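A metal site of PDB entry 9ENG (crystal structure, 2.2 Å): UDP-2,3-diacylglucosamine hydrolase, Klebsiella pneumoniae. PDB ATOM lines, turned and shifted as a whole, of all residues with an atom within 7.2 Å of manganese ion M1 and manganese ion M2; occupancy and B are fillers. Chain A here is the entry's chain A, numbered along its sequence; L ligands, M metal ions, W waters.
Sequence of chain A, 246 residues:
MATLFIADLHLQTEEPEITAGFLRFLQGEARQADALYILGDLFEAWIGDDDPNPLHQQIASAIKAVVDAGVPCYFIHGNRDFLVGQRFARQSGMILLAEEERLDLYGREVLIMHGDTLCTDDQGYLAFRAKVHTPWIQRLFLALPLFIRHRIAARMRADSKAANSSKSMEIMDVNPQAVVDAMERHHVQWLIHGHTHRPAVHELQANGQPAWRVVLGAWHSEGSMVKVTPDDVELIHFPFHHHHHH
ND2 of Asn 79 sits at hydrogen-bond distance from O3 of the ligand.
A ring nitrogen (ND1) of His 10 is in hydrogen-bond range of the side-chain carboxylate (OE1) of Glu 44 (2.7 Å). A ring nitrogen (ND1) of His 114 is in hydrogen-bond range of the backbone carbonyl oxygen of Leu 39, 2.6 Å away. O of Asp 41 sits at hydrogen-bond distance from N of Leu 9, at 3.0 Å. The backbone carbonyl oxygen (O) of His 114 is in hydrogen-bond range of the backbone NH (N) of Gly 194, 2.8 Å away. The side-chain carboxylate of Asp 8 is in hydrogen-bond range of the backbone NH of His 195 (2.7 Å). The backbone NH (N) of Arg 80 lies within hydrogen-bond range of the side-chain carboxylate (OD1) of Asp 41 (3.2 Å). The backbone carbonyl oxygen (O) of Gly 40 lies within hydrogen-bond range of the backbone NH (N) of Asp 8, at 2.9 Å. The side-chain carboxylate (OD1) of Asp 81 lies within hydrogen-bond range of the backbone NH (N) of Asp 41 (3.0 Å).
Of the 23 residues printed, 4 come within 4 Å of manganese ion M1.
Within 4 Å of manganese ion M2: Asp 8, Asp 41, Asn 79, His 114 and His 195. The nearest printed residue that does not touch manganese ion M2 is His 10 (4.9 Å).
The side-chain carboxylate (OD1) of Asp 8 binds manganese ion M1 (2.1 Å). Water W1 is bound to manganese ion M1, 2.1 Å away. Manganese ion M1 is bound by a ring nitrogen (NE2) of His 10, at 2.2 Å. OD2 of Asp 41 is bound to manganese ion M1. Manganese ion M1 is bound by a ring nitrogen (NE2) of His 197, 2.2 Å away.
Manganese ion M2 is bound by OD2 of Asp 41 (2.1 Å), OD1 of Asn 79 (2.2 Å), water W1 (2.2 Å), ND1 of His 195 (2.2 Å) and NE2 of His 114 (2.2 Å). Manganese ion M2 has five donor atoms within binding distance.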
ATOM      1  N   ALA A   7      16.086   0.332 -20.304  1.00  0.00           N
ATOM      2  CA  ALA A   7      14.946  -0.400 -20.818  1.00  0.00           C
ATOM      3  C   ALA A   7      13.680   0.271 -20.325  1.00  0.00           C
ATOM      4  O   ALA A   7      13.727   1.084 -19.402  1.00  0.00           O
ATOM      5  CB  ALA A   7      15.009  -1.840 -20.417  1.00  0.00           C
ATOM      6  N   ASP A   8      12.545  -0.037 -20.948  1.00  0.00           N
ATOM      7  CA  ASP A   8      11.250   0.221 -20.327  1.00  0.00           C
ATOM      8  C   ASP A   8      10.980   1.711 -20.208  1.00  0.00           C
ATOM      9  O   ASP A   8      10.352   2.176 -19.262  1.00  0.00           O
ATOM     10  CB  ASP A   8      11.152  -0.527 -18.998  1.00  0.00           C
ATOM     11  CG  ASP A   8      11.128  -2.036 -19.201  1.00  0.00           C
ATOM     12  OD1 ASP A   8      10.176  -2.495 -19.794  1.00  0.00           O
ATOM     13  OD2 ASP A   8      12.093  -2.728 -18.828  1.00  0.00           O
ATOM     14  N   LEU A   9      11.415   2.468 -21.218  1.00  0.00           N
ATOM     15  CA  LEU A   9      11.078   3.875 -21.293  1.00  0.00           C
ATOM     16  C   LEU A   9       9.601   4.100 -21.664  1.00  0.00           C
ATOM     17  O   LEU A   9       9.034   5.138 -21.318  1.00  0.00           O
ATOM     18  CB  LEU A   9      12.014   4.521 -22.312  1.00  0.00           C
ATOM     19  CG  LEU A   9      13.472   4.652 -21.837  1.00  0.00           C
ATOM     20  CD1 LEU A   9      14.289   3.412 -22.185  1.00  0.00           C
ATOM     21  CD2 LEU A   9      14.095   5.888 -22.440  1.00  0.00           C
ATOM     22  N   HIS A  10       8.987   3.134 -22.371  1.00  0.00           N
ATOM     23  CA  HIS A  10       7.589   3.216 -22.801  1.00  0.00           C
ATOM     24  C   HIS A  10       7.235   4.586 -23.350  1.00  0.00           C
ATOM     25  O   HIS A  10       6.286   5.224 -22.905  1.00  0.00           O
ATOM     26  CB  HIS A  10       6.648   2.815 -21.658  1.00  0.00           C
ATOM     27  CG  HIS A  10       6.768   1.380 -21.267  1.00  0.00           C
ATOM     28  ND1 HIS A  10       5.950   0.371 -21.723  1.00  0.00           N
ATOM     29  CD2 HIS A  10       7.673   0.787 -20.475  1.00  0.00           C
ATOM     30  CE1 HIS A  10       6.336  -0.783 -21.209  1.00  0.00           C
ATOM     31  NE2 HIS A  10       7.373  -0.545 -20.430  1.00  0.00           N
ATOM     32  N   LEU A  39      17.317  -2.438 -23.778  1.00  0.00           N
ATOM     33  CA  LEU A  39      16.799  -3.798 -23.667  1.00  0.00           C
ATOM     34  C   LEU A  39      15.275  -3.846 -23.717  1.00  0.00           C
ATOM     35  O   LEU A  39      14.656  -4.565 -22.936  1.00  0.00           O
ATOM     36  CB  LEU A  39      17.319  -4.425 -22.372  1.00  0.00           C
ATOM     37  CG  LEU A  39      18.829  -4.331 -22.149  1.00  0.00           C
ATOM     38  CD1 LEU A  39      19.233  -5.217 -20.985  1.00  0.00           C
ATOM     39  CD2 LEU A  39      19.593  -4.706 -23.405  1.00  0.00           C
ATOM     40  N   GLY A  40      14.666  -3.090 -24.656  1.00  0.00           N
ATOM     41  CA  GLY A  40      13.288  -3.296 -25.059  1.00  0.00           C
ATOM     42  C   GLY A  40      12.326  -2.367 -24.323  1.00  0.00           C
ATOM     43  O   GLY A  40      12.685  -1.809 -23.289  1.00  0.00           O
ATOM     44  N   ASP A  41      11.115  -2.232 -24.869  1.00  0.00           N
ATOM     45  CA  ASP A  41      10.095  -1.302 -24.417  1.00  0.00           C
ATOM     46  C   ASP A  41      10.664   0.123 -24.431  1.00  0.00           C
ATOM     47  O   ASP A  41      10.407   0.939 -23.541  1.00  0.00           O
ATOM     48  CB  ASP A  41       9.547  -1.691 -23.041  1.00  0.00           C
ATOM     49  CG  ASP A  41       8.707  -2.960 -23.022  1.00  0.00           C
ATOM     50  OD1 ASP A  41       8.549  -3.562 -24.117  1.00  0.00           O
ATOM     51  OD2 ASP A  41       8.226  -3.335 -21.906  1.00  0.00           O
ATOM     52  N   LEU A  42      11.382   0.446 -25.489  1.00  0.00           N
ATOM     53  CA  LEU A  42      11.698   1.830 -25.758  1.00  0.00           C
ATOM     54  C   LEU A  42      10.409   2.583 -26.042  1.00  0.00           C
ATOM     55  O   LEU A  42      10.240   3.736 -25.636  1.00  0.00           O
ATOM     56  CB  LEU A  42      12.671   1.892 -26.944  1.00  0.00           C
ATOM     57  CG  LEU A  42      13.165   3.277 -27.344  1.00  0.00           C
ATOM     58  CD1 LEU A  42      13.857   3.988 -26.182  1.00  0.00           C
ATOM     59  CD2 LEU A  42      14.121   3.161 -28.504  1.00  0.00           C
ATOM     60  N   GLU A  44       6.019   2.595 -26.148  1.00  0.00           N
ATOM     61  CA  GLU A  44       4.820   2.074 -25.506  1.00  0.00           C
ATOM     62  C   GLU A  44       4.051   1.148 -26.468  1.00  0.00           C
ATOM     63  O   GLU A  44       3.315   0.272 -26.026  1.00  0.00           O
ATOM     64  CB  GLU A  44       3.895   3.225 -25.122  1.00  0.00           C
ATOM     65  CG  GLU A  44       2.574   2.798 -24.474  1.00  0.00           C
ATOM     66  CD  GLU A  44       2.693   1.695 -23.434  1.00  0.00           C
ATOM     67  OE1 GLU A  44       3.828   1.377 -23.025  1.00  0.00           O
ATOM     68  OE2 GLU A  44       1.643   1.147 -23.035  1.00  0.00           O
ATOM     69  N   GLY A  78      11.268  -5.524 -26.923  1.00  0.00           N
ATOM     70  CA  GLY A  78      10.393  -5.906 -25.838  1.00  0.00           C
ATOM     71  C   GLY A  78       9.051  -6.410 -26.367  1.00  0.00           C
ATOM     72  O   GLY A  78       8.887  -6.561 -27.565  1.00  0.00           O
ATOM     73  N   ASN A  79       8.139  -6.680 -25.440  1.00  0.00           N
ATOM     74  CA  ASN A  79       6.806  -7.142 -25.768  1.00  0.00           C
ATOM     75  C   ASN A  79       5.994  -6.001 -26.414  1.00  0.00           C
ATOM     76  O   ASN A  79       5.042  -6.264 -27.142  1.00  0.00           O
ATOM     77  CB  ASN A  79       6.109  -7.707 -24.523  1.00  0.00           C
ATOM     78  CG  ASN A  79       6.006  -6.725 -23.374  1.00  0.00           C
ATOM     79  OD1 ASN A  79       6.995  -6.460 -22.696  1.00  0.00           O
ATOM     80  ND2 ASN A  79       4.821  -6.203 -23.125  1.00  0.00           N
ATOM     81  N   ARG A  80       6.356  -4.738 -26.115  1.00  0.00           N
ATOM     82  CA  ARG A  80       5.583  -3.602 -26.590  1.00  0.00           C
ATOM     83  C   ARG A  80       6.003  -3.249 -28.013  1.00  0.00           C
ATOM     84  O   ARG A  80       5.160  -2.812 -28.792  1.00  0.00           O
ATOM     85  CB  ARG A  80       5.701  -2.349 -25.713  1.00  0.00           C
ATOM     86  CG  ARG A  80       5.263  -2.525 -24.249  1.00  0.00           C
ATOM     87  CD  ARG A  80       3.826  -2.946 -23.985  1.00  0.00           C
ATOM     88  NE  ARG A  80       2.907  -2.081 -24.704  1.00  0.00           N
ATOM     89  CZ  ARG A  80       1.596  -2.242 -24.762  1.00  0.00           C
ATOM     90  NH1 ARG A  80       0.991  -3.087 -23.961  1.00  0.00           N
ATOM     91  NH2 ARG A  80       0.897  -1.508 -25.623  1.00  0.00           N
ATOM     92  N   ASP A  81       7.294  -3.421 -28.335  1.00  0.00           N
ATOM     93  CA  ASP A  81       7.875  -2.860 -29.547  1.00  0.00           C
ATOM     94  C   ASP A  81       8.618  -3.915 -30.383  1.00  0.00           C
ATOM     95  O   ASP A  81       9.543  -3.576 -31.134  1.00  0.00           O
ATOM     96  CB  ASP A  81       8.763  -1.656 -29.237  1.00  0.00           C
ATOM     97  CG  ASP A  81       9.758  -1.825 -28.098  1.00  0.00           C
ATOM     98  OD1 ASP A  81       9.907  -2.961 -27.552  1.00  0.00           O
ATOM     99  OD2 ASP A  81      10.412  -0.830 -27.789  1.00  0.00           O
ATOM    100  N   HIS A 114      15.277  -8.812 -22.751  1.00  0.00           N
ATOM    101  CA  HIS A 114      14.254  -7.890 -22.304  1.00  0.00           C
ATOM    102  C   HIS A 114      13.740  -8.340 -20.940  1.00  0.00           C
ATOM    103  O   HIS A 114      13.464  -7.512 -20.072  1.00  0.00           O
ATOM    104  CB  HIS A 114      13.074  -7.743 -23.277  1.00  0.00           C
ATOM    105  CG  HIS A 114      11.993  -6.860 -22.731  1.00  0.00           C
ATOM    106  ND1 HIS A 114      12.264  -5.530 -22.502  1.00  0.00           N
ATOM    107  CD2 HIS A 114      10.717  -7.055 -22.379  1.00  0.00           C
ATOM    108  CE1 HIS A 114      11.167  -4.949 -22.019  1.00  0.00           C
ATOM    109  NE2 HIS A 114      10.211  -5.844 -21.946  1.00  0.00           N
ATOM    110  N   GLY A 115      13.540  -9.652 -20.822  1.00  0.00           N
ATOM    111  CA  GLY A 115      13.151 -10.241 -19.556  1.00  0.00           C
ATOM    112  C   GLY A 115      11.815 -10.959 -19.620  1.00  0.00           C
ATOM    113  O   GLY A 115      11.488 -11.751 -18.734  1.00  0.00           O
ATOM    114  N   ASP A 116      11.023 -10.681 -20.665  1.00  0.00           N
ATOM    115  CA  ASP A 116       9.680 -11.222 -20.735  1.00  0.00           C
ATOM    116  C   ASP A 116       9.693 -12.729 -20.988  1.00  0.00           C
ATOM    117  O   ASP A 116       8.742 -13.416 -20.610  1.00  0.00           O
ATOM    118  CB  ASP A 116       8.829 -10.502 -21.791  1.00  0.00           C
ATOM    119  CG  ASP A 116       9.385 -10.625 -23.190  1.00  0.00           C
ATOM    120  OD1 ASP A 116       8.677 -11.172 -24.061  1.00  0.00           O
ATOM    121  OD2 ASP A 116      10.523 -10.170 -23.402  1.00  0.00           O
ATOM    122  N   TYR A 125       0.346 -14.878 -21.703  1.00  0.00           N
ATOM    123  CA  TYR A 125       1.242 -14.000 -22.437  1.00  0.00           C
ATOM    124  C   TYR A 125       2.099 -14.819 -23.395  1.00  0.00           C
ATOM    125  O   TYR A 125       2.449 -14.343 -24.469  1.00  0.00           O
ATOM    126  CB  TYR A 125       2.168 -13.201 -21.518  1.00  0.00           C
ATOM    127  CG  TYR A 125       3.298 -12.542 -22.276  1.00  0.00           C
ATOM    128  CD1 TYR A 125       3.077 -11.413 -23.047  1.00  0.00           C
ATOM    129  CD2 TYR A 125       4.573 -13.090 -22.282  1.00  0.00           C
ATOM    130  CE1 TYR A 125       4.089 -10.814 -23.763  1.00  0.00           C
ATOM    131  CE2 TYR A 125       5.600 -12.512 -22.999  1.00  0.00           C
ATOM    132  CZ  TYR A 125       5.347 -11.371 -23.744  1.00  0.00           C
ATOM    133  OH  TYR A 125       6.325 -10.762 -24.469  1.00  0.00           O
ATOM    134  N   ILE A 171       2.403  -6.589 -13.845  1.00  0.00           N
ATOM    135  CA  ILE A 171       3.281  -7.394 -14.683  1.00  0.00           C
ATOM    136  C   ILE A 171       3.824  -8.574 -13.880  1.00  0.00           C
ATOM    137  O   ILE A 171       4.531  -8.394 -12.891  1.00  0.00           O
ATOM    138  CB  ILE A 171       4.418  -6.508 -15.241  1.00  0.00           C
ATOM    139  CG1 ILE A 171       3.867  -5.345 -16.072  1.00  0.00           C
ATOM    140  CG2 ILE A 171       5.432  -7.334 -16.015  1.00  0.00           C
ATOM    141  CD1 ILE A 171       4.940  -4.362 -16.495  1.00  0.00           C
ATOM    142  N   GLY A 194      15.055  -6.063 -18.230  1.00  0.00           N
ATOM    143  CA  GLY A 194      14.024  -5.183 -17.735  1.00  0.00           C
ATOM    144  C   GLY A 194      12.693  -5.917 -17.607  1.00  0.00           C
ATOM    145  O   GLY A 194      12.625  -7.033 -17.067  1.00  0.00           O
ATOM    146  N   HIS A 195      11.678  -5.301 -18.217  1.00  0.00           N
ATOM    147  CA  HIS A 195      10.347  -5.881 -18.431  1.00  0.00           C
ATOM    148  C   HIS A 195       9.514  -5.940 -17.159  1.00  0.00           C
ATOM    149  O   HIS A 195       8.321  -5.648 -17.219  1.00  0.00           O
ATOM    150  CB  HIS A 195      10.382  -7.282 -19.067  1.00  0.00           C
ATOM    151  CG  HIS A 195       9.008  -7.808 -19.233  1.00  0.00           C
ATOM    152  ND1 HIS A 195       8.041  -7.214 -20.020  1.00  0.00           N
ATOM    153  CD2 HIS A 195       8.415  -8.842 -18.606  1.00  0.00           C
ATOM    154  CE1 HIS A 195       6.909  -7.905 -19.887  1.00  0.00           C
ATOM    155  NE2 HIS A 195       7.111  -8.899 -19.033  1.00  0.00           N
ATOM    156  N   THR A 196      10.070  -6.441 -16.056  1.00  0.00           N
ATOM    157  CA  THR A 196       9.277  -6.661 -14.845  1.00  0.00           C
ATOM    158  C   THR A 196       8.975  -5.350 -14.114  1.00  0.00           C
ATOM    159  O   THR A 196       8.091  -5.305 -13.247  1.00  0.00           O
ATOM    160  CB  THR A 196       9.992  -7.619 -13.878  1.00  0.00           C
ATOM    161  OG1 THR A 196      11.237  -7.044 -13.518  1.00  0.00           O
ATOM    162  CG2 THR A 196      10.268  -8.993 -14.443  1.00  0.00           C
ATOM    163  N   HIS A 197       9.749  -4.294 -14.387  1.00  0.00           N
ATOM    164  CA  HIS A 197       9.540  -2.963 -13.809  1.00  0.00           C
ATOM    165  C   HIS A 197       9.854  -2.923 -12.306  1.00  0.00           C
ATOM    166  O   HIS A 197       9.514  -1.945 -11.653  1.00  0.00           O
ATOM    167  CB  HIS A 197       8.135  -2.430 -14.128  1.00  0.00           C
ATOM    168  CG  HIS A 197       7.899  -2.132 -15.568  1.00  0.00           C
ATOM    169  ND1 HIS A 197       6.795  -1.443 -16.028  1.00  0.00           N
ATOM    170  CD2 HIS A 197       8.656  -2.374 -16.650  1.00  0.00           C
ATOM    171  CE1 HIS A 197       6.905  -1.276 -17.337  1.00  0.00           C
ATOM    172  NE2 HIS A 197       8.047  -1.822 -17.732  1.00  0.00           N
ATOM    173  N   ALA A 218      11.329   0.855 -15.005  1.00  0.00           N
ATOM    174  CA  ALA A 218      10.618   1.699 -15.962  1.00  0.00           C
ATOM    175  C   ALA A 218      10.902   3.180 -15.733  1.00  0.00           C
ATOM    176  O   ALA A 218      11.239   3.609 -14.630  1.00  0.00           O
ATOM    177  CB  ALA A 218       9.136   1.411 -15.861  1.00  0.00           C
HETATM  178  C1  LIG L   1      -1.494  -8.378 -34.636  1.00  0.00           C
HETATM  179  C2  LIG L   1      -1.306  -7.254 -33.812  1.00  0.00           C
HETATM  180  C3  LIG L   1      -0.011  -6.811 -33.560  1.00  0.00           C
HETATM  181  C4  LIG L   1       1.025  -7.562 -34.038  1.00  0.00           C
HETATM  182  C5  LIG L   1       0.790  -8.676 -34.823  1.00  0.00           C
HETATM  183  C6  LIG L   1      -0.462  -9.116 -35.148  1.00  0.00           C
HETATM  184  N1  LIG L   1       0.248  -5.707 -32.701  1.00  0.00           N
HETATM  185  C7  LIG L   1       1.507  -5.045 -32.826  1.00  0.00           C
HETATM  186  C8  LIG L   1       1.787  -4.345 -31.501  1.00  0.00           C
HETATM  187  C9  LIG L   1      -0.819  -4.710 -32.700  1.00  0.00           C
HETATM  188  C10 LIG L   1      -0.700  -3.864 -31.396  1.00  0.00           C
HETATM  189  N2  LIG L   1       0.725  -3.317 -31.183  1.00  0.00           N
HETATM  190  S1  LIG L   1       0.973  -2.476 -29.774  1.00  0.00           S
HETATM  191  C11 LIG L   1       0.791  -3.612 -28.487  1.00  0.00           C
HETATM  192  O1  LIG L   1       2.320  -2.001 -29.783  1.00  0.00           O
HETATM  193  O2  LIG L   1      -0.102  -1.533 -29.648  1.00  0.00           O
HETATM  194  C12 LIG L   1      -0.432  -3.730 -27.864  1.00  0.00           C
HETATM  195  C13 LIG L   1      -0.623  -4.669 -26.880  1.00  0.00           C
HETATM  196  C14 LIG L   1       0.413  -5.495 -26.513  1.00  0.00           C
HETATM  197  C15 LIG L   1       1.828  -4.467 -28.137  1.00  0.00           C
HETATM  198  C16 LIG L   1       1.629  -5.421 -27.164  1.00  0.00           C
HETATM  199  N3  LIG L   1       0.168  -6.461 -25.547  1.00  0.00           N
HETATM  200  C17 LIG L   1       1.130  -6.920 -24.707  1.00  0.00           C
HETATM  201  O3  LIG L   1       2.278  -6.481 -24.767  1.00  0.00           O
HETATM  202  C18 LIG L   1       0.741  -8.007 -23.706  1.00  0.00           C
HETATM  203  C19 LIG L   1      -0.052  -9.084 -24.139  1.00  0.00           C
HETATM  204  C20 LIG L   1      -0.447 -10.082 -23.245  1.00  0.00           C
HETATM  205  C21 LIG L   1      -0.073 -10.020 -21.916  1.00  0.00           C
HETATM  206  C22 LIG L   1       0.723  -8.956 -21.466  1.00  0.00           C
HETATM  207  C23 LIG L   1       1.113  -7.937 -22.348  1.00  0.00           C
HETATM  208  N4  LIG L   1       1.085  -8.914 -20.060  1.00  0.00           N
HETATM  209  S2  LIG L   1       2.662  -8.834 -19.559  1.00  0.00           S
HETATM  210  C24 LIG L   1       3.352 -10.470 -19.383  1.00  0.00           C
HETATM  211  O4  LIG L   1       3.411  -8.121 -20.558  1.00  0.00           O
HETATM  212  O5  LIG L   1       2.638  -8.309 -18.237  1.00  0.00           O
HETATM  213 CL1  LIG L   1       2.121  -9.528 -35.443  1.00  0.00          CL
HETATM  214 CL2  LIG L   1      -3.084  -8.877 -35.069  1.00  0.00          CL
HETATM  215 MN    MN M   1       8.084  -2.524 -19.860  1.00  0.00          MN
HETATM  216 MN    MN M   2       8.136  -5.367 -21.232  1.00  0.00          MN
HETATM  217  O   HOH W   1       7.383  -4.490 -19.357  1.00  0.00           O
